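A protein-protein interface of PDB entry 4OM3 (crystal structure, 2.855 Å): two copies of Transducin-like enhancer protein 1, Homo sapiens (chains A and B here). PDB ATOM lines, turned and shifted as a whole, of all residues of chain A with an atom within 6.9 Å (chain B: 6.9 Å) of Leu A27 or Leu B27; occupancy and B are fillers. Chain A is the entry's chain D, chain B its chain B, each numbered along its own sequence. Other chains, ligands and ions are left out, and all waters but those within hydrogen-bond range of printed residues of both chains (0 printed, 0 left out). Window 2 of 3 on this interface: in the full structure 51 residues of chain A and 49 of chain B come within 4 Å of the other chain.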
ATOM      1  N   LYS A  21      -3.913 -15.548  -1.032  1.00  0.00           N
ATOM      2  CA  LYS A  21      -4.327 -16.066   0.269  1.00  0.00           C
ATOM      3  C   LYS A  21      -4.899 -14.948   1.135  1.00  0.00           C
ATOM      4  O   LYS A  21      -6.029 -15.037   1.580  1.00  0.00           O
ATOM      5  CB  LYS A  21      -3.168 -16.773   0.987  1.00  0.00           C
ATOM      6  CG  LYS A  21      -3.610 -17.669   2.144  1.00  0.00           C
ATOM      7  CD  LYS A  21      -2.449 -18.066   3.059  1.00  0.00           C
ATOM      8  CE  LYS A  21      -1.338 -18.814   2.323  1.00  0.00           C
ATOM      9  NZ  LYS A  21      -1.762 -20.134   1.786  1.00  0.00           N
ATOM     10  N   GLU A  22      -4.116 -13.891   1.343  1.00  0.00           N
ATOM     11  CA  GLU A  22      -4.547 -12.703   2.091  1.00  0.00           C
ATOM     12  C   GLU A  22      -5.948 -12.204   1.720  1.00  0.00           C
ATOM     13  O   GLU A  22      -6.801 -12.008   2.594  1.00  0.00           O
ATOM     14  CB  GLU A  22      -3.542 -11.559   1.905  1.00  0.00           C
ATOM     15  CG  GLU A  22      -2.232 -11.731   2.667  1.00  0.00           C
ATOM     16  CD  GLU A  22      -1.262 -10.578   2.449  1.00  0.00           C
ATOM     17  OE1 GLU A  22      -1.421  -9.827   1.460  1.00  0.00           O
ATOM     18  OE2 GLU A  22      -0.333 -10.421   3.270  1.00  0.00           O
ATOM     19  N   GLU A  23      -6.181 -11.991   0.428  1.00  0.00           N
ATOM     20  CA  GLU A  23      -7.494 -11.548  -0.037  1.00  0.00           C
ATOM     21  C   GLU A  23      -8.577 -12.576   0.295  1.00  0.00           C
ATOM     22  O   GLU A  23      -9.677 -12.214   0.731  1.00  0.00           O
ATOM     23  CB  GLU A  23      -7.473 -11.234  -1.536  1.00  0.00           C
ATOM     24  CG  GLU A  23      -6.616 -10.025  -1.895  1.00  0.00           C
ATOM     25  CD  GLU A  23      -6.785  -9.588  -3.338  1.00  0.00           C
ATOM     26  OE1 GLU A  23      -6.149  -8.589  -3.737  1.00  0.00           O
ATOM     27  OE2 GLU A  23      -7.556 -10.238  -4.073  1.00  0.00           O
ATOM     28  N   PHE A  24      -8.263 -13.858   0.116  1.00  0.00           N
ATOM     29  CA  PHE A  24      -9.244 -14.904   0.404  1.00  0.00           C
ATOM     30  C   PHE A  24      -9.616 -14.987   1.890  1.00  0.00           C
ATOM     31  O   PHE A  24     -10.793 -15.068   2.237  1.00  0.00           O
ATOM     32  CB  PHE A  24      -8.771 -16.268  -0.102  1.00  0.00           C
ATOM     33  CG  PHE A  24      -9.851 -17.311  -0.111  1.00  0.00           C
ATOM     34  CD1 PHE A  24     -10.012 -18.173   0.961  1.00  0.00           C
ATOM     35  CD2 PHE A  24     -10.717 -17.418  -1.187  1.00  0.00           C
ATOM     36  CE1 PHE A  24     -11.012 -19.128   0.957  1.00  0.00           C
ATOM     37  CE2 PHE A  24     -11.717 -18.371  -1.199  1.00  0.00           C
ATOM     38  CZ  PHE A  24     -11.866 -19.227  -0.124  1.00  0.00           C
ATOM     39  N   GLN A  25      -8.605 -14.977   2.754  1.00  0.00           N
ATOM     40  CA  GLN A  25      -8.792 -14.976   4.201  1.00  0.00           C
ATOM     41  C   GLN A  25      -9.602 -13.757   4.619  1.00  0.00           C
ATOM     42  O   GLN A  25     -10.478 -13.845   5.488  1.00  0.00           O
ATOM     43  CB  GLN A  25      -7.436 -14.970   4.919  1.00  0.00           C
ATOM     44  CG  GLN A  25      -6.623 -16.250   4.758  1.00  0.00           C
ATOM     45  CD  GLN A  25      -5.252 -16.163   5.409  1.00  0.00           C
ATOM     46  OE1 GLN A  25      -4.725 -15.073   5.633  1.00  0.00           O
ATOM     47  NE2 GLN A  25      -4.667 -17.317   5.715  1.00  0.00           N
ATOM     48  N   PHE A  26      -9.301 -12.622   3.994  1.00  0.00           N
ATOM     49  CA  PHE A  26     -10.051 -11.396   4.235  1.00  0.00           C
ATOM     50  C   PHE A  26     -11.527 -11.595   3.914  1.00  0.00           C
ATOM     51  O   PHE A  26     -12.398 -11.210   4.696  1.00  0.00           O
ATOM     52  CB  PHE A  26      -9.488 -10.239   3.407  1.00  0.00           C
ATOM     53  CG  PHE A  26     -10.245  -8.950   3.577  1.00  0.00           C
ATOM     54  CD1 PHE A  26      -9.956  -8.098   4.630  1.00  0.00           C
ATOM     55  CD2 PHE A  26     -11.244  -8.593   2.686  1.00  0.00           C
ATOM     56  CE1 PHE A  26     -10.651  -6.914   4.793  1.00  0.00           C
ATOM     57  CE2 PHE A  26     -11.943  -7.411   2.844  1.00  0.00           C
ATOM     58  CZ  PHE A  26     -11.645  -6.570   3.898  1.00  0.00           C
ATOM     59  N   LEU A  27     -11.806 -12.197   2.760  1.00  0.00           N
ATOM     60  CA  LEU A  27     -13.188 -12.433   2.352  1.00  0.00           C
ATOM     61  C   LEU A  27     -13.898 -13.411   3.291  1.00  0.00           C
ATOM     62  O   LEU A  27     -15.093 -13.270   3.561  1.00  0.00           O
ATOM     63  CB  LEU A  27     -13.253 -12.931   0.906  1.00  0.00           C
ATOM     64  CG  LEU A  27     -14.655 -13.051   0.304  1.00  0.00           C
ATOM     65  CD1 LEU A  27     -15.448 -11.775   0.539  1.00  0.00           C
ATOM     66  CD2 LEU A  27     -14.573 -13.360  -1.180  1.00  0.00           C
ATOM     67  N   GLN A  28     -13.155 -14.397   3.784  1.00  0.00           N
ATOM     68  CA  GLN A  28     -13.681 -15.356   4.750  1.00  0.00           C
ATOM     69  C   GLN A  28     -14.113 -14.629   6.023  1.00  0.00           C
ATOM     70  O   GLN A  28     -15.234 -14.814   6.518  1.00  0.00           O
ATOM     71  CB  GLN A  28     -12.622 -16.415   5.068  1.00  0.00           C
ATOM     72  CG  GLN A  28     -13.073 -17.511   6.022  1.00  0.00           C
ATOM     73  CD  GLN A  28     -12.043 -18.619   6.164  1.00  0.00           C
ATOM     74  OE1 GLN A  28     -11.117 -18.729   5.359  1.00  0.00           O
ATOM     75  NE2 GLN A  28     -12.200 -19.448   7.190  1.00  0.00           N
ATOM     76  N   ALA A  29     -13.216 -13.788   6.535  1.00  0.00           N
ATOM     77  CA  ALA A  29     -13.501 -12.979   7.715  1.00  0.00           C
ATOM     78  C   ALA A  29     -14.735 -12.104   7.504  1.00  0.00           C
ATOM     79  O   ALA A  29     -15.639 -12.067   8.347  1.00  0.00           O
ATOM     80  CB  ALA A  29     -12.297 -12.119   8.066  1.00  0.00           C
ATOM     81  N   GLN A  30     -14.766 -11.410   6.369  1.00  0.00           N
ATOM     82  CA  GLN A  30     -15.889 -10.548   6.018  1.00  0.00           C
ATOM     83  C   GLN A  30     -17.211 -11.307   6.007  1.00  0.00           C
ATOM     84  O   GLN A  30     -18.210 -10.832   6.554  1.00  0.00           O
ATOM     85  CB  GLN A  30     -15.656  -9.875   4.663  1.00  0.00           C
ATOM     86  CG  GLN A  30     -14.918  -8.550   4.754  1.00  0.00           C
ATOM     87  CD  GLN A  30     -15.702  -7.500   5.518  1.00  0.00           C
ATOM     88  OE1 GLN A  30     -16.933  -7.482   5.490  1.00  0.00           O
ATOM     89  NE2 GLN A  30     -14.990  -6.620   6.214  1.00  0.00           N
ATOM     90  N   TYR A  31     -17.214 -12.486   5.390  1.00  0.00           N
ATOM     91  CA  TYR A  31     -18.423 -13.300   5.350  1.00  0.00           C
ATOM     92  C   TYR A  31     -18.850 -13.731   6.748  1.00  0.00           C
ATOM     93  O   TYR A  31     -20.043 -13.790   7.043  1.00  0.00           O
ATOM     94  CB  TYR A  31     -18.251 -14.530   4.455  1.00  0.00           C
ATOM     95  CG  TYR A  31     -19.487 -15.405   4.423  1.00  0.00           C
ATOM     96  CD1 TYR A  31     -20.545 -15.114   3.571  1.00  0.00           C
ATOM     97  CD2 TYR A  31     -19.605 -16.511   5.256  1.00  0.00           C
ATOM     98  CE1 TYR A  31     -21.679 -15.904   3.542  1.00  0.00           C
ATOM     99  CE2 TYR A  31     -20.735 -17.306   5.236  1.00  0.00           C
ATOM    100  CZ  TYR A  31     -21.769 -16.998   4.377  1.00  0.00           C
ATOM    101  OH  TYR A  31     -22.895 -17.787   4.353  1.00  0.00           O
ATOM    102  N   HIS A  32     -17.877 -14.039   7.603  1.00  0.00           N
ATOM    103  CA  HIS A  32     -18.195 -14.424   8.977  1.00  0.00           C
ATOM    104  C   HIS A  32     -18.883 -13.283   9.729  1.00  0.00           C
ATOM    105  O   HIS A  32     -19.974 -13.458  10.296  1.00  0.00           O
ATOM    106  CB  HIS A  32     -16.937 -14.866   9.724  1.00  0.00           C
ATOM    107  CG  HIS A  32     -17.216 -15.497  11.053  1.00  0.00           C
ATOM    108  ND1 HIS A  32     -17.755 -16.759  11.178  1.00  0.00           N
ATOM    109  CD2 HIS A  32     -17.036 -15.038  12.315  1.00  0.00           C
ATOM    110  CE1 HIS A  32     -17.891 -17.052  12.460  1.00  0.00           C
ATOM    111  NE2 HIS A  32     -17.463 -16.025  13.169  1.00  0.00           N
ATOM    112  N   LYS B  21     -10.251 -20.591  -8.191  1.00  0.00           N
ATOM    113  CA  LYS B  21     -11.156 -19.623  -8.799  1.00  0.00           C
ATOM    114  C   LYS B  21     -12.610 -19.994  -8.517  1.00  0.00           C
ATOM    115  O   LYS B  21     -13.411 -19.146  -8.112  1.00  0.00           O
ATOM    116  CB  LYS B  21     -10.922 -19.535 -10.309  1.00  0.00           C
ATOM    117  CG  LYS B  21     -11.556 -18.314 -10.961  1.00  0.00           C
ATOM    118  CD  LYS B  21     -11.754 -18.513 -12.456  1.00  0.00           C
ATOM    119  CE  LYS B  21     -10.450 -18.855 -13.158  1.00  0.00           C
ATOM    120  NZ  LYS B  21     -10.659 -19.102 -14.613  1.00  0.00           N
ATOM    121  N   GLU B  22     -12.938 -21.267  -8.722  1.00  0.00           N
ATOM    122  CA  GLU B  22     -14.289 -21.763  -8.472  1.00  0.00           C
ATOM    123  C   GLU B  22     -14.724 -21.525  -7.027  1.00  0.00           C
ATOM    124  O   GLU B  22     -15.809 -20.989  -6.774  1.00  0.00           O
ATOM    125  CB  GLU B  22     -14.386 -23.252  -8.812  1.00  0.00           C
ATOM    126  N   GLU B  23     -13.870 -21.914  -6.082  1.00  0.00           N
ATOM    127  CA  GLU B  23     -14.188 -21.758  -4.665  1.00  0.00           C
ATOM    128  C   GLU B  23     -14.341 -20.292  -4.255  1.00  0.00           C
ATOM    129  O   GLU B  23     -15.236 -19.944  -3.479  1.00  0.00           O
ATOM    130  CB  GLU B  23     -13.145 -22.460  -3.791  1.00  0.00           C
ATOM    131  CG  GLU B  23     -13.106 -23.970  -3.976  1.00  0.00           C
ATOM    132  CD  GLU B  23     -12.325 -24.675  -2.885  1.00  0.00           C
ATOM    133  OE1 GLU B  23     -11.905 -24.002  -1.922  1.00  0.00           O
ATOM    134  OE2 GLU B  23     -12.134 -25.906  -2.989  1.00  0.00           O
ATOM    135  N   PHE B  24     -13.469 -19.438  -4.783  1.00  0.00           N
ATOM    136  CA  PHE B  24     -13.541 -18.006  -4.507  1.00  0.00           C
ATOM    137  C   PHE B  24     -14.849 -17.404  -5.014  1.00  0.00           C
ATOM    138  O   PHE B  24     -15.574 -16.744  -4.262  1.00  0.00           O
ATOM    139  CB  PHE B  24     -12.349 -17.278  -5.131  1.00  0.00           C
ATOM    140  CG  PHE B  24     -12.527 -15.789  -5.217  1.00  0.00           C
ATOM    141  CD1 PHE B  24     -12.388 -14.994  -4.091  1.00  0.00           C
ATOM    142  CD2 PHE B  24     -12.825 -15.184  -6.427  1.00  0.00           C
ATOM    143  CE1 PHE B  24     -12.549 -13.622  -4.170  1.00  0.00           C
ATOM    144  CE2 PHE B  24     -12.987 -13.814  -6.512  1.00  0.00           C
ATOM    145  CZ  PHE B  24     -12.848 -13.032  -5.382  1.00  0.00           C
ATOM    146  N   GLN B  25     -15.139 -17.635  -6.293  1.00  0.00           N
ATOM    147  CA  GLN B  25     -16.374 -17.153  -6.907  1.00  0.00           C
ATOM    148  C   GLN B  25     -17.595 -17.629  -6.126  1.00  0.00           C
ATOM    149  O   GLN B  25     -18.543 -16.868  -5.913  1.00  0.00           O
ATOM    150  CB  GLN B  25     -16.461 -17.604  -8.368  1.00  0.00           C
ATOM    151  CG  GLN B  25     -15.437 -16.948  -9.279  1.00  0.00           C
ATOM    152  CD  GLN B  25     -15.469 -17.498 -10.691  1.00  0.00           C
ATOM    153  OE1 GLN B  25     -16.184 -18.457 -10.981  1.00  0.00           O
ATOM    154  NE2 GLN B  25     -14.689 -16.893 -11.580  1.00  0.00           N
ATOM    155  N   PHE B  26     -17.557 -18.887  -5.696  1.00  0.00           N
ATOM    156  CA  PHE B  26     -18.590 -19.437  -4.823  1.00  0.00           C
ATOM    157  C   PHE B  26     -18.754 -18.583  -3.564  1.00  0.00           C
ATOM    158  O   PHE B  26     -19.838 -18.053  -3.288  1.00  0.00           O
ATOM    159  CB  PHE B  26     -18.238 -20.879  -4.444  1.00  0.00           C
ATOM    160  CG  PHE B  26     -19.164 -21.486  -3.429  1.00  0.00           C
ATOM    161  CD1 PHE B  26     -20.378 -22.027  -3.815  1.00  0.00           C
ATOM    162  CD2 PHE B  26     -18.814 -21.523  -2.088  1.00  0.00           C
ATOM    163  CE1 PHE B  26     -21.231 -22.586  -2.883  1.00  0.00           C
ATOM    164  CE2 PHE B  26     -19.664 -22.080  -1.152  1.00  0.00           C
ATOM    165  CZ  PHE B  26     -20.873 -22.613  -1.550  1.00  0.00           C
ATOM    166  N   LEU B  27     -17.662 -18.449  -2.817  1.00  0.00           N
ATOM    167  CA  LEU B  27     -17.638 -17.706  -1.562  1.00  0.00           C
ATOM    168  C   LEU B  27     -18.203 -16.294  -1.695  1.00  0.00           C
ATOM    169  O   LEU B  27     -19.041 -15.877  -0.883  1.00  0.00           O
ATOM    170  CB  LEU B  27     -16.206 -17.652  -1.020  1.00  0.00           C
ATOM    171  CG  LEU B  27     -15.971 -16.825   0.242  1.00  0.00           C
ATOM    172  CD1 LEU B  27     -16.818 -17.346   1.389  1.00  0.00           C
ATOM    173  CD2 LEU B  27     -14.494 -16.827   0.614  1.00  0.00           C
ATOM    174  N   GLN B  28     -17.754 -15.564  -2.715  1.00  0.00           N
ATOM    175  CA  GLN B  28     -18.200 -14.186  -2.920  1.00  0.00           C
ATOM    176  C   GLN B  28     -19.639 -14.083  -3.419  1.00  0.00           C
ATOM    177  O   GLN B  28     -20.331 -13.107  -3.128  1.00  0.00           O
ATOM    178  CB  GLN B  28     -17.255 -13.424  -3.861  1.00  0.00           C
ATOM    179  CG  GLN B  28     -17.159 -14.007  -5.264  1.00  0.00           C
ATOM    180  CD  GLN B  28     -16.475 -13.080  -6.254  1.00  0.00           C
ATOM    181  OE1 GLN B  28     -16.317 -11.884  -6.002  1.00  0.00           O
ATOM    182  NE2 GLN B  28     -16.073 -13.630  -7.394  1.00  0.00           N
ATOM    183  N   ALA B  29     -20.085 -15.073  -4.185  1.00  0.00           N
ATOM    184  CA  ALA B  29     -21.487 -15.121  -4.586  1.00  0.00           C
ATOM    185  C   ALA B  29     -22.340 -15.246  -3.324  1.00  0.00           C
ATOM    186  O   ALA B  29     -23.353 -14.544  -3.156  1.00  0.00           O
ATOM    187  CB  ALA B  29     -21.742 -16.288  -5.505  1.00  0.00           C
ATOM    188  N   GLN B  30     -21.910 -16.139  -2.434  1.00  0.00           N
ATOM    189  CA  GLN B  30     -22.576 -16.329  -1.152  1.00  0.00           C
ATOM    190  C   GLN B  30     -22.576 -15.049  -0.316  1.00  0.00           C
ATOM    191  O   GLN B  30     -23.580 -14.720   0.322  1.00  0.00           O
ATOM    192  CB  GLN B  30     -21.924 -17.480  -0.382  1.00  0.00           C
ATOM    193  CG  GLN B  30     -21.988 -18.812  -1.113  1.00  0.00           C
ATOM    194  CD  GLN B  30     -23.372 -19.105  -1.661  1.00  0.00           C
ATOM    195  OE1 GLN B  30     -24.332 -19.254  -0.906  1.00  0.00           O
ATOM    196  NE2 GLN B  30     -23.481 -19.178  -2.984  1.00  0.00           N
ATOM    197  N   TYR B  31     -21.456 -14.328  -0.325  1.00  0.00           N
ATOM    198  CA  TYR B  31     -21.370 -13.068   0.410  1.00  0.00           C
ATOM    199  C   TYR B  31     -22.339 -12.032  -0.150  1.00  0.00           C
ATOM    200  O   TYR B  31     -22.986 -11.307   0.603  1.00  0.00           O
ATOM    201  CB  TYR B  31     -19.941 -12.516   0.406  1.00  0.00           C
ATOM    202  CG  TYR B  31     -19.812 -11.159   1.071  1.00  0.00           C
ATOM    203  CD1 TYR B  31     -19.646 -11.050   2.447  1.00  0.00           C
ATOM    204  CD2 TYR B  31     -19.858  -9.988   0.323  1.00  0.00           C
ATOM    205  CE1 TYR B  31     -19.531  -9.812   3.057  1.00  0.00           C
ATOM    206  CE2 TYR B  31     -19.745  -8.749   0.924  1.00  0.00           C
ATOM    207  CZ  TYR B  31     -19.581  -8.667   2.291  1.00  0.00           C
ATOM    208  OH  TYR B  31     -19.467  -7.433   2.891  1.00  0.00           O
ATOM    209  N   HIS B  32     -22.425 -11.961  -1.475  1.00  0.00           N
ATOM    210  CA  HIS B  32     -23.349 -11.048  -2.140  1.00  0.00           C
ATOM    211  C   HIS B  32     -24.795 -11.345  -1.749  1.00  0.00           C
ATOM    212  O   HIS B  32     -25.546 -10.440  -1.357  1.00  0.00           O
ATOM    213  CB  HIS B  32     -23.182 -11.133  -3.659  1.00  0.00           C
ATOM    214  CG  HIS B  32     -24.392 -10.698  -4.425  1.00  0.00           C
ATOM    215  ND1 HIS B  32     -24.964  -9.453  -4.274  1.00  0.00           N
ATOM    216  CD2 HIS B  32     -25.136 -11.343  -5.353  1.00  0.00           C
ATOM    217  CE1 HIS B  32     -26.010  -9.352  -5.074  1.00  0.00           C
ATOM    218  NE2 HIS B  32     -26.137 -10.485  -5.740  1.00  0.00           N
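Phe B24 touches Phe A24.
Phe A24 touches Leu B27.
Phe B24 touches Leu A27.
Leu A27 touches Leu B27 (CG to CD2, 3.8 Å).
Leu A27 touches Gln B28 (CD2 to CB, 3.8 Å).
Gln A30 touches Tyr B31 (OE1 to OH, 3.6 Å).
Gln B30 touches Tyr A31.
Tyr A31 touches Tyr B31.
Hydrophobic or aromatic side chains of chain A that line the printed part of chain B: Phe A24, Leu A27 and Tyr A31.
Of the 12 printed residues of chain B, 5 touch a printed residue of chain A.
Printed residues of chain B that touch a printed residue of chain A: Phe B24, Leu B27, Gln B28, Gln B30 and Tyr B31.
Hydrophobic or aromatic side chains of chain B that line the printed part of chain A: Phe B24, Leu B27 and Tyr B31.
Among the printed residues, 8 pairs touch across the chains.
Among the printed residues, no Asp or Glu carboxylate lies within 4 Å of a Lys or Arg side-chain nitrogen of the other chain.
Of chain A, only Phe A24 (3.6 Å) and Leu A27 (3.8 Å) come within 4 Å of Leu B27.
Of the printed residues of chain B, Tyr A31 touches Gln B30 and Tyr B31.
Of the printed residues of chain A, Tyr B31 touches Gln A30 and Tyr A31.
Of the printed residues of chain A, Gln B28 touches Leu A27 (3.8 Å).
Of the printed residues of chain A, Phe B24 touches Phe A24 (3.8 Å) and Leu A27 (3.6 Å).
The nearest residue of chain B that does not touch Leu A27 is Tyr B31 (4.4 Å).
The nearest residue of chain A that does not touch Leu B27 is Gln A28 (4.2 Å).
The nearest printed residue of chain A that does not touch Gln B30 is Leu A27 (7.9 Å).
Phe B24 touches its own counterpart, Phe A24.
Leu A27 touches its own counterpart, Leu B27.
Leu A27 touches Gln B28, but with the chains exchanged Gln A28 does not touch Leu B27 (4.2 Å).
Gln A30 touches Tyr B31, and with the chains exchanged Tyr A31 touches Gln B30.
Of the 8 pairs that touch across the chains among the printed residues, 7 have their exchanged pair printed and touching as well.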
